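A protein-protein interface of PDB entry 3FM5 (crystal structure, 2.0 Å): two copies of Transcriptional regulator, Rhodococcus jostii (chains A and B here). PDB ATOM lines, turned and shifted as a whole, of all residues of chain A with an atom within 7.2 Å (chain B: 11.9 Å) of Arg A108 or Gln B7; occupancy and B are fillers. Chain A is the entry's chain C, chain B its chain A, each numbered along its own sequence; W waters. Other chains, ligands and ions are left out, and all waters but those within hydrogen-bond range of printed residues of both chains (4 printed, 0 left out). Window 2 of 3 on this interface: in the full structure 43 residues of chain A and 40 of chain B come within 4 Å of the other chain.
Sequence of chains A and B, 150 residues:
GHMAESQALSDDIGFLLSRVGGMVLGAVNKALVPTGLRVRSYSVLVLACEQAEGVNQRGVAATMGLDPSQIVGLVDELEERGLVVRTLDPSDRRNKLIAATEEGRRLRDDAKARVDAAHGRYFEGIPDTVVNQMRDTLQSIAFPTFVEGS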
ATOM      1  N   LEU A  37      21.882  -6.448  23.121  1.00  0.00           N
ATOM      2  CA  LEU A  37      21.675  -7.125  21.846  1.00  0.00           C
ATOM      3  C   LEU A  37      21.444  -8.620  22.011  1.00  0.00           C
ATOM      4  O   LEU A  37      21.713  -9.195  23.069  1.00  0.00           O
ATOM      5  CB  LEU A  37      22.890  -6.921  20.936  1.00  0.00           C
ATOM      6  CG  LEU A  37      23.195  -5.487  20.512  1.00  0.00           C
ATOM      7  CD1 LEU A  37      24.539  -5.425  19.806  1.00  0.00           C
ATOM      8  CD2 LEU A  37      22.069  -4.956  19.626  1.00  0.00           C
ATOM      9  N   TYR A  42      22.131  -8.200  16.794  1.00  0.00           N
ATOM     10  CA  TYR A  42      23.569  -8.039  16.590  1.00  0.00           C
ATOM     11  C   TYR A  42      23.951  -8.260  15.123  1.00  0.00           C
ATOM     12  O   TYR A  42      24.720  -7.492  14.544  1.00  0.00           O
ATOM     13  CB  TYR A  42      24.347  -9.010  17.477  1.00  0.00           C
ATOM     14  CG  TYR A  42      25.804  -9.162  17.085  1.00  0.00           C
ATOM     15  CD1 TYR A  42      26.740  -8.182  17.408  1.00  0.00           C
ATOM     16  CD2 TYR A  42      26.243 -10.286  16.398  1.00  0.00           C
ATOM     17  CE1 TYR A  42      28.071  -8.318  17.053  1.00  0.00           C
ATOM     18  CE2 TYR A  42      27.577 -10.431  16.034  1.00  0.00           C
ATOM     19  CZ  TYR A  42      28.482  -9.446  16.363  1.00  0.00           C
ATOM     20  OH  TYR A  42      29.802  -9.587  16.006  1.00  0.00           O
ATOM     21  N   LEU A  45      22.991  -5.360  12.975  1.00  0.00           N
ATOM     22  CA  LEU A  45      23.925  -4.263  13.198  1.00  0.00           C
ATOM     23  C   LEU A  45      25.217  -4.505  12.423  1.00  0.00           C
ATOM     24  O   LEU A  45      25.760  -3.588  11.805  1.00  0.00           O
ATOM     25  CB  LEU A  45      24.218  -4.100  14.691  1.00  0.00           C
ATOM     26  CG  LEU A  45      25.134  -2.946  15.091  1.00  0.00           C
ATOM     27  CD1 LEU A  45      24.617  -1.622  14.535  1.00  0.00           C
ATOM     28  CD2 LEU A  45      25.278  -2.889  16.610  1.00  0.00           C
ATOM     29  N   VAL A  46      25.700  -5.747  12.451  1.00  0.00           N
ATOM     30  CA  VAL A  46      26.918  -6.111  11.735  1.00  0.00           C
ATOM     31  C   VAL A  46      26.757  -5.868  10.234  1.00  0.00           C
ATOM     32  O   VAL A  46      27.645  -5.320   9.583  1.00  0.00           O
ATOM     33  CB  VAL A  46      27.307  -7.581  11.978  1.00  0.00           C
ATOM     34  CG1 VAL A  46      28.419  -8.010  11.014  1.00  0.00           C
ATOM     35  CG2 VAL A  46      27.737  -7.777  13.420  1.00  0.00           C
ATOM     36  N   LEU A  47      25.615  -6.275   9.692  1.00  0.00           N
ATOM     37  CA  LEU A  47      25.331  -6.051   8.280  1.00  0.00           C
ATOM     38  C   LEU A  47      25.311  -4.557   7.979  1.00  0.00           C
ATOM     39  O   LEU A  47      25.898  -4.105   6.998  1.00  0.00           O
ATOM     40  CB  LEU A  47      24.003  -6.701   7.887  1.00  0.00           C
ATOM     41  CG  LEU A  47      24.041  -8.234   7.879  1.00  0.00           C
ATOM     42  CD1 LEU A  47      22.699  -8.821   7.489  1.00  0.00           C
ATOM     43  CD2 LEU A  47      25.134  -8.729   6.944  1.00  0.00           C
ATOM     44  N   CYS A  49      26.839  -2.267   9.507  1.00  0.00           N
ATOM     45  CA  CYS A  49      28.174  -1.703   9.691  1.00  0.00           C
ATOM     46  C   CYS A  49      29.141  -2.064   8.564  1.00  0.00           C
ATOM     47  O   CYS A  49      30.217  -1.478   8.464  1.00  0.00           O
ATOM     48  CB  CYS A  49      28.775  -2.148  11.029  1.00  0.00           C
ATOM     49  SG  CYS A  49      28.104  -1.318  12.481  1.00  0.00           S
ATOM     50  N   GLU A  50      28.762  -3.023   7.723  1.00  0.00           N
ATOM     51  CA  GLU A  50      29.661  -3.520   6.681  1.00  0.00           C
ATOM     52  C   GLU A  50      30.037  -2.455   5.654  1.00  0.00           C
ATOM     53  O   GLU A  50      31.181  -2.398   5.204  1.00  0.00           O
ATOM     54  CB  GLU A  50      29.069  -4.748   5.984  1.00  0.00           C
ATOM     55  CG  GLU A  50      29.178  -6.024   6.804  1.00  0.00           C
ATOM     56  CD  GLU A  50      28.551  -7.223   6.112  1.00  0.00           C
ATOM     57  OE1 GLU A  50      28.664  -8.348   6.652  1.00  0.00           O
ATOM     58  OE2 GLU A  50      27.945  -7.033   5.031  1.00  0.00           O
ATOM     59  N   LEU A  83      21.173   3.369  17.202  1.00  0.00           N
ATOM     60  CA  LEU A  83      22.316   2.584  16.762  1.00  0.00           C
ATOM     61  C   LEU A  83      22.303   2.496  15.248  1.00  0.00           C
ATOM     62  O   LEU A  83      23.291   2.124  14.613  1.00  0.00           O
ATOM     63  CB  LEU A  83      22.237   1.179  17.353  1.00  0.00           C
ATOM     64  CG  LEU A  83      22.119   1.140  18.876  1.00  0.00           C
ATOM     65  CD1 LEU A  83      21.826  -0.271  19.359  1.00  0.00           C
ATOM     66  CD2 LEU A  83      23.395   1.676  19.499  1.00  0.00           C
ATOM     67  N   ALA A 100      24.401   2.322   9.977  1.00  0.00           N
ATOM     68  CA  ALA A 100      24.823   2.362  11.371  1.00  0.00           C
ATOM     69  C   ALA A 100      25.246   3.771  11.773  1.00  0.00           C
ATOM     70  O   ALA A 100      25.875   4.481  10.990  1.00  0.00           O
ATOM     71  CB  ALA A 100      25.961   1.382  11.607  1.00  0.00           C
ATOM     72  N   GLU A 102      27.384   6.256  14.628  1.00  0.00           N
ATOM     73  CA  GLU A 102      28.681   6.119  15.243  1.00  0.00           C
ATOM     74  C   GLU A 102      28.538   5.325  16.501  1.00  0.00           C
ATOM     75  O   GLU A 102      29.354   4.514  16.799  1.00  0.00           O
ATOM     76  CB  GLU A 102      29.283   7.477  15.564  1.00  0.00           C
ATOM     77  CG  GLU A 102      29.913   8.178  14.386  1.00  0.00           C
ATOM     78  CD  GLU A 102      30.525   7.226  13.345  1.00  0.00           C
ATOM     79  OE1 GLU A 102      31.571   6.610  13.630  1.00  0.00           O
ATOM     80  OE2 GLU A 102      29.969   7.105  12.223  1.00  0.00           O
ATOM     81  N   GLU A 103      27.477   5.567  17.238  1.00  0.00           N
ATOM     82  CA  GLU A 103      27.214   4.767  18.409  1.00  0.00           C
ATOM     83  C   GLU A 103      27.001   3.298  18.084  1.00  0.00           C
ATOM     84  O   GLU A 103      27.505   2.447  18.750  1.00  0.00           O
ATOM     85  CB  GLU A 103      26.023   5.284  19.160  1.00  0.00           C
ATOM     86  CG  GLU A 103      25.985   4.772  20.549  1.00  0.00           C
ATOM     87  CD  GLU A 103      24.851   5.338  21.282  1.00  0.00           C
ATOM     88  OE1 GLU A 103      24.308   6.288  20.757  1.00  0.00           O
ATOM     89  OE2 GLU A 103      24.483   4.839  22.353  1.00  0.00           O
ATOM     90  N   GLY A 104      26.260   3.033  17.028  1.00  0.00           N
ATOM     91  CA  GLY A 104      26.020   1.685  16.590  1.00  0.00           C
ATOM     92  C   GLY A 104      27.323   1.020  16.293  1.00  0.00           C
ATOM     93  O   GLY A 104      27.536  -0.125  16.619  1.00  0.00           O
ATOM     94  N   ARG A 105      28.215   1.766  15.681  1.00  0.00           N
ATOM     95  CA  ARG A 105      29.517   1.208  15.333  1.00  0.00           C
ATOM     96  C   ARG A 105      30.325   0.894  16.586  1.00  0.00           C
ATOM     97  O   ARG A 105      31.031  -0.113  16.641  1.00  0.00           O
ATOM     98  CB  ARG A 105      30.293   2.162  14.418  1.00  0.00           C
ATOM     99  CG  ARG A 105      29.656   2.321  13.043  1.00  0.00           C
ATOM    100  CD  ARG A 105      30.588   2.996  12.043  1.00  0.00           C
ATOM    101  NE  ARG A 105      29.934   3.137  10.745  1.00  0.00           N
ATOM    102  CZ  ARG A 105      29.853   2.167   9.839  1.00  0.00           C
ATOM    103  NH1 ARG A 105      29.228   2.384   8.690  1.00  0.00           N
ATOM    104  NH2 ARG A 105      30.393   0.980  10.083  1.00  0.00           N
ATOM    105  N   ARG A 106      30.226   1.761  17.591  1.00  0.00           N
ATOM    106  CA  ARG A 106      30.907   1.516  18.858  1.00  0.00           C
ATOM    107  C   ARG A 106      30.350   0.273  19.538  1.00  0.00           C
ATOM    108  O   ARG A 106      31.105  -0.570  20.020  1.00  0.00           O
ATOM    109  CB  ARG A 106      30.822   2.734  19.791  1.00  0.00           C
ATOM    110  CG  ARG A 106      32.087   3.587  19.797  1.00  0.00           C
ATOM    111  CD  ARG A 106      31.975   4.812  20.705  1.00  0.00           C
ATOM    112  NE  ARG A 106      31.431   5.956  19.981  1.00  0.00           N
ATOM    113  CZ  ARG A 106      30.279   6.551  20.265  1.00  0.00           C
ATOM    114  NH1 ARG A 106      29.540   6.131  21.283  1.00  0.00           N
ATOM    115  NH2 ARG A 106      29.873   7.580  19.535  1.00  0.00           N
ATOM    116  N   LEU A 107      29.026   0.150  19.557  1.00  0.00           N
ATOM    117  CA  LEU A 107      28.385  -1.015  20.163  1.00  0.00           C
ATOM    118  C   LEU A 107      28.726  -2.288  19.404  1.00  0.00           C
ATOM    119  O   LEU A 107      28.983  -3.333  20.003  1.00  0.00           O
ATOM    120  CB  LEU A 107      26.871  -0.840  20.222  1.00  0.00           C
ATOM    121  CG  LEU A 107      26.172  -1.883  21.094  1.00  0.00           C
ATOM    122  CD1 LEU A 107      26.500  -1.632  22.574  1.00  0.00           C
ATOM    123  CD2 LEU A 107      24.673  -1.868  20.855  1.00  0.00           C
ATOM    124  N   ARG A 108      28.727  -2.202  18.079  1.00  0.00           N
ATOM    125  CA  ARG A 108      29.082  -3.352  17.259  1.00  0.00           C
ATOM    126  C   ARG A 108      30.500  -3.813  17.598  1.00  0.00           C
ATOM    127  O   ARG A 108      30.755  -5.012  17.715  1.00  0.00           O
ATOM    128  CB  ARG A 108      28.951  -3.017  15.769  1.00  0.00           C
ATOM    129  CG  ARG A 108      29.109  -4.212  14.833  1.00  0.00           C
ATOM    130  CD  ARG A 108      30.567  -4.630  14.686  1.00  0.00           C
ATOM    131  NE  ARG A 108      31.259  -3.917  13.617  1.00  0.00           N
ATOM    132  CZ  ARG A 108      31.789  -2.704  13.739  1.00  0.00           C
ATOM    133  NH1 ARG A 108      31.696  -2.046  14.885  1.00  0.00           N
ATOM    134  NH2 ARG A 108      32.408  -2.141  12.710  1.00  0.00           N
ATOM    135  N   ASP A 109      31.416  -2.860  17.761  1.00  0.00           N
ATOM    136  CA  ASP A 109      32.791  -3.182  18.135  1.00  0.00           C
ATOM    137  C   ASP A 109      32.852  -3.863  19.499  1.00  0.00           C
ATOM    138  O   ASP A 109      33.578  -4.839  19.683  1.00  0.00           O
ATOM    139  CB  ASP A 109      33.652  -1.918  18.158  1.00  0.00           C
ATOM    140  CG  ASP A 109      34.190  -1.552  16.791  1.00  0.00           C
ATOM    141  OD1 ASP A 109      34.031  -2.359  15.849  1.00  0.00           O
ATOM    142  OD2 ASP A 109      34.781  -0.458  16.663  1.00  0.00           O
ATOM    143  N   ASP A 110      32.101  -3.335  20.458  1.00  0.00           N
ATOM    144  CA  ASP A 110      32.038  -3.937  21.787  1.00  0.00           C
ATOM    145  C   ASP A 110      31.440  -5.344  21.733  1.00  0.00           C
ATOM    146  O   ASP A 110      31.943  -6.262  22.379  1.00  0.00           O
ATOM    147  CB  ASP A 110      31.222  -3.059  22.740  1.00  0.00           C
ATOM    148  CG  ASP A 110      31.107  -3.659  24.131  1.00  0.00           C
ATOM    149  OD1 ASP A 110      32.124  -3.705  24.854  1.00  0.00           O
ATOM    150  OD2 ASP A 110      29.997  -4.083  24.507  1.00  0.00           O
ATOM    151  N   ALA A 111      30.364  -5.505  20.966  1.00  0.00           N
ATOM    152  CA  ALA A 111      29.657  -6.784  20.886  1.00  0.00           C
ATOM    153  C   ALA A 111      30.514  -7.864  20.232  1.00  0.00           C
ATOM    154  O   ALA A 111      30.544  -9.004  20.698  1.00  0.00           O
ATOM    155  CB  ALA A 111      28.330  -6.628  20.139  1.00  0.00           C
ATOM    156  N   LYS A 112      31.218  -7.493  19.166  1.00  0.00           N
ATOM    157  CA  LYS A 112      32.097  -8.418  18.457  1.00  0.00           C
ATOM    158  C   LYS A 112      33.153  -9.009  19.395  1.00  0.00           C
ATOM    159  O   LYS A 112      33.471 -10.197  19.318  1.00  0.00           O
ATOM    160  CB  LYS A 112      32.764  -7.712  17.268  1.00  0.00           C
ATOM    161  CG  LYS A 112      33.848  -8.516  16.547  1.00  0.00           C
ATOM    162  CD  LYS A 112      33.256  -9.584  15.645  1.00  0.00           C
ATOM    163  CE  LYS A 112      34.132  -9.837  14.415  1.00  0.00           C
ATOM    164  NZ  LYS A 112      35.441 -10.468  14.733  1.00  0.00           N
ATOM    165  N   ALA A 113      33.696  -8.179  20.280  1.00  0.00           N
ATOM    166  CA  ALA A 113      34.683  -8.650  21.244  1.00  0.00           C
ATOM    167  C   ALA A 113      34.070  -9.753  22.101  1.00  0.00           C
ATOM    168  O   ALA A 113      34.689 -10.795  22.342  1.00  0.00           O
ATOM    169  CB  ALA A 113      35.157  -7.504  22.116  1.00  0.00           C
ATOM    170  N   ARG A 114      32.842  -9.517  22.552  1.00  0.00           N
ATOM    171  CA  ARG A 114      32.129 -10.481  23.380  1.00  0.00           C
ATOM    172  C   ARG A 114      31.786 -11.744  22.589  1.00  0.00           C
ATOM    173  O   ARG A 114      31.910 -12.860  23.097  1.00  0.00           O
ATOM    174  CB  ARG A 114      30.861  -9.848  23.966  1.00  0.00           C
ATOM    175  CG  ARG A 114      31.159  -8.650  24.867  1.00  0.00           C
ATOM    176  CD  ARG A 114      29.902  -7.994  25.405  1.00  0.00           C
ATOM    177  NE  ARG A 114      30.230  -6.735  26.069  1.00  0.00           N
ATOM    178  CZ  ARG A 114      30.562  -6.633  27.353  1.00  0.00           C
ATOM    179  NH1 ARG A 114      30.597  -7.718  28.115  1.00  0.00           N
ATOM    180  NH2 ARG A 114      30.855  -5.447  27.874  1.00  0.00           N
ATOM    181  N   VAL A 115      31.350 -11.568  21.349  1.00  0.00           N
ATOM    182  CA  VAL A 115      31.005 -12.721  20.520  1.00  0.00           C
ATOM    183  C   VAL A 115      32.236 -13.594  20.275  1.00  0.00           C
ATOM    184  O   VAL A 115      32.177 -14.815  20.426  1.00  0.00           O
ATOM    185  CB  VAL A 115      30.362 -12.310  19.178  1.00  0.00           C
ATOM    186  CG1 VAL A 115      30.255 -13.510  18.251  1.00  0.00           C
ATOM    187  CG2 VAL A 115      28.985 -11.698  19.411  1.00  0.00           C
ATOM    188  N   ASP A 116      33.350 -12.962  19.914  1.00  0.00           N
ATOM    189  CA  ASP A 116      34.601 -13.680  19.688  1.00  0.00           C
ATOM    190  C   ASP A 116      35.050 -14.462  20.916  1.00  0.00           C
ATOM    191  O   ASP A 116      35.472 -15.610  20.803  1.00  0.00           O
ATOM    192  CB  ASP A 116      35.705 -12.719  19.244  1.00  0.00           C
ATOM    193  CG  ASP A 116      35.524 -12.256  17.818  1.00  0.00           C
ATOM    194  OD1 ASP A 116      36.135 -11.238  17.436  1.00  0.00           O
ATOM    195  OD2 ASP A 116      34.760 -12.914  17.082  1.00  0.00           O
ATOM    196  N   MET B   3      37.067 -14.129   8.819  1.00  0.00           N
ATOM    197  CA  MET B   3      37.742 -15.403   9.002  1.00  0.00           C
ATOM    198  C   MET B   3      38.985 -15.249   9.880  1.00  0.00           C
ATOM    199  O   MET B   3      39.686 -16.225  10.152  1.00  0.00           O
ATOM    200  CB  MET B   3      38.117 -16.004   7.645  1.00  0.00           C
ATOM    201  N   ALA B   4      39.250 -14.021  10.319  1.00  0.00           N
ATOM    202  CA  ALA B   4      40.391 -13.734  11.189  1.00  0.00           C
ATOM    203  C   ALA B   4      40.129 -12.488  12.033  1.00  0.00           C
ATOM    204  O   ALA B   4      39.919 -12.576  13.243  1.00  0.00           O
ATOM    205  CB  ALA B   4      41.658 -13.565  10.365  1.00  0.00           C
ATOM    206  N   GLU B   5      40.154 -11.327  11.386  1.00  0.00           N
ATOM    207  CA  GLU B   5      39.758 -10.080  12.027  1.00  0.00           C
ATOM    208  C   GLU B   5      38.633  -9.475  11.184  1.00  0.00           C
ATOM    209  O   GLU B   5      38.298  -8.295  11.295  1.00  0.00           O
ATOM    210  CB  GLU B   5      40.962  -9.141  12.173  1.00  0.00           C
ATOM    211  CG  GLU B   5      40.977  -7.919  11.271  1.00  0.00           C
ATOM    212  CD  GLU B   5      40.511  -6.667  11.996  1.00  0.00           C
ATOM    213  OE1 GLU B   5      40.074  -6.784  13.160  1.00  0.00           O
ATOM    214  OE2 GLU B   5      40.585  -5.568  11.407  1.00  0.00           O
ATOM    215  N   SER B   6      38.044 -10.326  10.350  1.00  0.00           N
ATOM    216  CA  SER B   6      36.948  -9.944   9.466  1.00  0.00           C
ATOM    217  C   SER B   6      35.757  -9.343  10.202  1.00  0.00           C
ATOM    218  O   SER B   6      35.435  -9.738  11.324  1.00  0.00           O
ATOM    219  CB  SER B   6      36.474 -11.152   8.661  1.00  0.00           C
ATOM    220  OG  SER B   6      35.195 -10.909   8.102  1.00  0.00           O
ATOM    221  N   GLN B   7      35.093  -8.401   9.543  1.00  0.00           N
ATOM    222  CA  GLN B   7      33.943  -7.738  10.140  1.00  0.00           C
ATOM    223  C   GLN B   7      32.659  -8.168   9.443  1.00  0.00           C
ATOM    224  O   GLN B   7      31.577  -7.681   9.757  1.00  0.00           O
ATOM    225  CB  GLN B   7      34.104  -6.218  10.073  1.00  0.00           C
ATOM    226  CG  GLN B   7      33.522  -5.483  11.270  1.00  0.00           C
ATOM    227  CD  GLN B   7      34.364  -5.656  12.521  1.00  0.00           C
ATOM    228  OE1 GLN B   7      35.595  -5.679  12.455  1.00  0.00           O
ATOM    229  NE2 GLN B   7      33.706  -5.773  13.669  1.00  0.00           N
ATOM    230  N   ALA B   8      32.782  -9.107   8.508  1.00  0.00           N
ATOM    231  CA  ALA B   8      31.635  -9.591   7.746  1.00  0.00           C
ATOM    232  C   ALA B   8      30.859 -10.689   8.470  1.00  0.00           C
ATOM    233  O   ALA B   8      31.443 -11.635   8.995  1.00  0.00           O
ATOM    234  CB  ALA B   8      32.082 -10.083   6.376  1.00  0.00           C
ATOM    235  N   LEU B   9      29.538 -10.558   8.473  1.00  0.00           N
ATOM    236  CA  LEU B   9      28.662 -11.567   9.049  1.00  0.00           C
ATOM    237  C   LEU B   9      28.884 -12.925   8.383  1.00  0.00           C
ATOM    238  O   LEU B   9      28.727 -13.974   9.014  1.00  0.00           O
ATOM    239  CB  LEU B   9      27.198 -11.146   8.897  1.00  0.00           C
ATOM    240  CG  LEU B   9      26.192 -12.028   9.638  1.00  0.00           C
ATOM    241  CD1 LEU B   9      26.377 -11.879  11.153  1.00  0.00           C
ATOM    242  CD2 LEU B   9      24.769 -11.687   9.230  1.00  0.00           C
ATOM    243  N   SER B  10      29.254 -12.902   7.104  1.00  0.00           N
ATOM    244  CA  SER B  10      29.457 -14.130   6.348  1.00  0.00           C
ATOM    245  C   SER B  10      30.668 -14.932   6.832  1.00  0.00           C
ATOM    246  O   SER B  10      30.866 -16.074   6.410  1.00  0.00           O
ATOM    247  CB  SER B  10      29.571 -13.833   4.845  1.00  0.00           C
ATOM    248  OG  SER B  10      30.605 -12.902   4.583  1.00  0.00           O
ATOM    249  N   ASP B  11      31.472 -14.337   7.713  1.00  0.00           N
ATOM    250  CA  ASP B  11      32.612 -15.031   8.312  1.00  0.00           C
ATOM    251  C   ASP B  11      32.342 -15.454   9.764  1.00  0.00           C
ATOM    252  O   ASP B  11      33.109 -16.218  10.350  1.00  0.00           O
ATOM    253  CB  ASP B  11      33.869 -14.156   8.249  1.00  0.00           C
ATOM    254  CG  ASP B  11      34.370 -13.956   6.829  1.00  0.00           C
ATOM    255  OD1 ASP B  11      34.869 -12.851   6.523  1.00  0.00           O
ATOM    256  OD2 ASP B  11      34.254 -14.899   6.016  1.00  0.00           O
ATOM    257  N   ASP B  12      31.253 -14.945  10.334  1.00  0.00           N
ATOM    258  CA  ASP B  12      30.858 -15.269  11.703  1.00  0.00           C
ATOM    259  C   ASP B  12      30.447 -16.740  11.790  1.00  0.00           C
ATOM    260  O   ASP B  12      29.376 -17.124  11.314  1.00  0.00           O
ATOM    261  CB  ASP B  12      29.707 -14.341  12.124  1.00  0.00           C
ATOM    262  CG  ASP B  12      29.164 -14.644  13.505  1.00  0.00           C
ATOM    263  OD1 ASP B  12      28.706 -13.687  14.168  1.00  0.00           O
ATOM    264  OD2 ASP B  12      29.180 -15.822  13.925  1.00  0.00           O
ATOM    265  N   ILE B  13      31.291 -17.555  12.418  1.00  0.00           N
ATOM    266  CA  ILE B  13      31.081 -19.005  12.445  1.00  0.00           C
ATOM    267  C   ILE B  13      29.800 -19.433  13.162  1.00  0.00           C
ATOM    268  O   ILE B  13      29.195 -20.432  12.795  1.00  0.00           O
ATOM    269  CB  ILE B  13      32.288 -19.760  13.055  1.00  0.00           C
ATOM    270  CG1 ILE B  13      32.157 -21.264  12.817  1.00  0.00           C
ATOM    271  CG2 ILE B  13      32.418 -19.471  14.543  1.00  0.00           C
ATOM    272  CD1 ILE B  13      32.298 -21.668  11.362  1.00  0.00           C
ATOM    273  N   PHE B  15      26.981 -17.594  13.266  1.00  0.00           N
ATOM    274  CA  PHE B  15      25.934 -17.290  12.301  1.00  0.00           C
ATOM    275  C   PHE B  15      25.815 -18.383  11.241  1.00  0.00           C
ATOM    276  O   PHE B  15      24.713 -18.830  10.912  1.00  0.00           O
ATOM    277  CB  PHE B  15      26.191 -15.947  11.620  1.00  0.00           C
ATOM    278  CG  PHE B  15      25.249 -15.667  10.484  1.00  0.00           C
ATOM    279  CD1 PHE B  15      23.944 -15.277  10.731  1.00  0.00           C
ATOM    280  CD2 PHE B  15      25.661 -15.823   9.171  1.00  0.00           C
ATOM    281  CE1 PHE B  15      23.068 -15.033   9.689  1.00  0.00           C
ATOM    282  CE2 PHE B  15      24.787 -15.579   8.120  1.00  0.00           C
ATOM    283  CZ  PHE B  15      23.490 -15.184   8.383  1.00  0.00           C
ATOM    284  N   LEU B  16      26.958 -18.805  10.710  1.00  0.00           N
ATOM    285  CA  LEU B  16      26.992 -19.819   9.656  1.00  0.00           C
ATOM    286  C   LEU B  16      26.416 -21.149  10.110  1.00  0.00           C
ATOM    287  O   LEU B  16      25.644 -21.775   9.379  1.00  0.00           O
ATOM    288  CB  LEU B  16      28.423 -20.031   9.155  1.00  0.00           C
ATOM    289  CG  LEU B  16      29.025 -18.885   8.350  1.00  0.00           C
ATOM    290  CD1 LEU B  16      30.514 -19.139   8.127  1.00  0.00           C
ATOM    291  CD2 LEU B  16      28.305 -18.717   7.018  1.00  0.00           C
HETATM  292  O   HOH W   1      30.449 -11.681  14.623  1.00  0.00           O
HETATM  293  O   HOH W   2      36.512 -12.929  12.991  1.00  0.00           O
HETATM  294  O   HOH W   3      30.334  -5.075  10.111  1.00  0.00           O
HETATM  295  O   HOH W   4      28.184 -10.550   5.337  1.00  0.00           O
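The backbone carbonyl oxygen of Ser B6 lies close to the side-chain amino group of Lys A112 (3.5 Å).
The guanidinium group (NE) of Arg A108 lies close to the side-chain amide nitrogen (NE2) of Gln B7.
N of Leu B9 sits at hydrogen-bond distance from OE1 of Glu A50, 3.0 Å away.
The backbone NH (N) of Ala B8 is in hydrogen-bond range of the side-chain hydroxyl (OG) of Ser B6, at 3.0 Å.
The side-chain carboxylate (OD1) of Asp B11 is in hydrogen-bond range of the side-chain hydroxyl (OG) of Ser B6.
The side-chain carboxylate of Asp B12 sits at hydrogen-bond distance from the backbone NH of Phe B15 (2.9 Å).
O of Arg A105 lies within hydrogen-bond range of NH1 of Arg A108 (2.7 Å).
OD1 of Asp A109 is in salt-bridge range of NH1 of Arg A108 (2.5 Å).
The side-chain amino group of Lys A112 is in salt-bridge range of the side-chain carboxylate of Asp A116, 2.9 Å away.
Among the printed residues, pairs that only touch across the chains: Glu A50 with Ala B8 (3.4 Å), Val A46 with Gln B7 (3.4 Å), Leu A47 with Leu B9 (3.7 Å), Val A46 with Leu B9 (3.8 Å), Tyr A42 with Asp B12 (3.9 Å) and Lys A112 with Gln B7 (3.98 Å).
Printed residues of chain B within 4 Å of Arg A108: Gln B7.
Of the printed residues of chain A, Gln B7 touches Val A46 (3.4 Å), Arg A108 (3.1 Å) and Lys A112 (3.98 Å).
Cys A49 touches none of the printed residues of chain B.
Glu A50 touches just these residues of chain B: Ala B8 and Leu B9.
No residue of chain B comes within 4 Å of Gly A104.
No residue of chain B comes within 4 Å of Arg A105.
No residue of chain B comes within 4 Å of Asp A110.
No residue of chain B comes within 4 Å of Ala A111.
Printed residues of chain A within 4 Å of Leu B9: Val A46 (3.8 Å), Leu A47 (3.7 Å) and Glu A50 (3.0 Å).
Of the printed residues of chain A, Ala B8 touches Glu A50.
Of the printed residues of chain B, Tyr A42 touches Asp B12 (3.9 Å).
The nearest printed residue of chain B that does not touch Arg A108 is Ala B8 (7.4 Å).
The nearest printed residue of chain A that does not touch Gln B7 is Asp A109 (4.1 Å).
Of the 24 printed residues of chain A, 6 touch a printed residue of chain B.
Hydrophobic or aromatic side chains of chain A that line the printed part of chain B: Tyr A42, Val A46 and Leu A47.
Of the 13 printed residues of chain B, 5 touch a printed residue of chain A.
Hydrophobic or aromatic side chains of chain B within 4 Å of the printed part of chain A: Ala B8 and Leu B9.
Along chain B the printed residues that touch a printed residue of chain A span positions 6 to 12.
Among the printed residues, no Asp or Glu carboxylate lies within 4 Å of a Lys or Arg side-chain nitrogen of the other chain.
No position is printed for both chains.
Of the 9 pairs that touch across the chains among the printed residues, none has its exchanged pair printed and touching as well.
Water W1 lies within hydrogen-bond range of OH of Tyr A42 (2.6 Å) and OD1 of Asp B12 (2.7 Å).
Water W4 lies within hydrogen-bond range of the side-chain carboxylate of Glu A50 (2.6 Å), the backbone NH of Ser B10 (3.1 Å) and the backbone NH of Leu B9 (3.4 Å).
Water W3 lies within hydrogen-bond range of the backbone carbonyl oxygen of Val A46 and the backbone carbonyl oxygen of Gln B7.
Water W2 lies within hydrogen-bond range of the side-chain amino group (NZ) of Lys A112 (3.2 Å) and the backbone carbonyl oxygen (O) of Ala B4 (3.4 Å).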
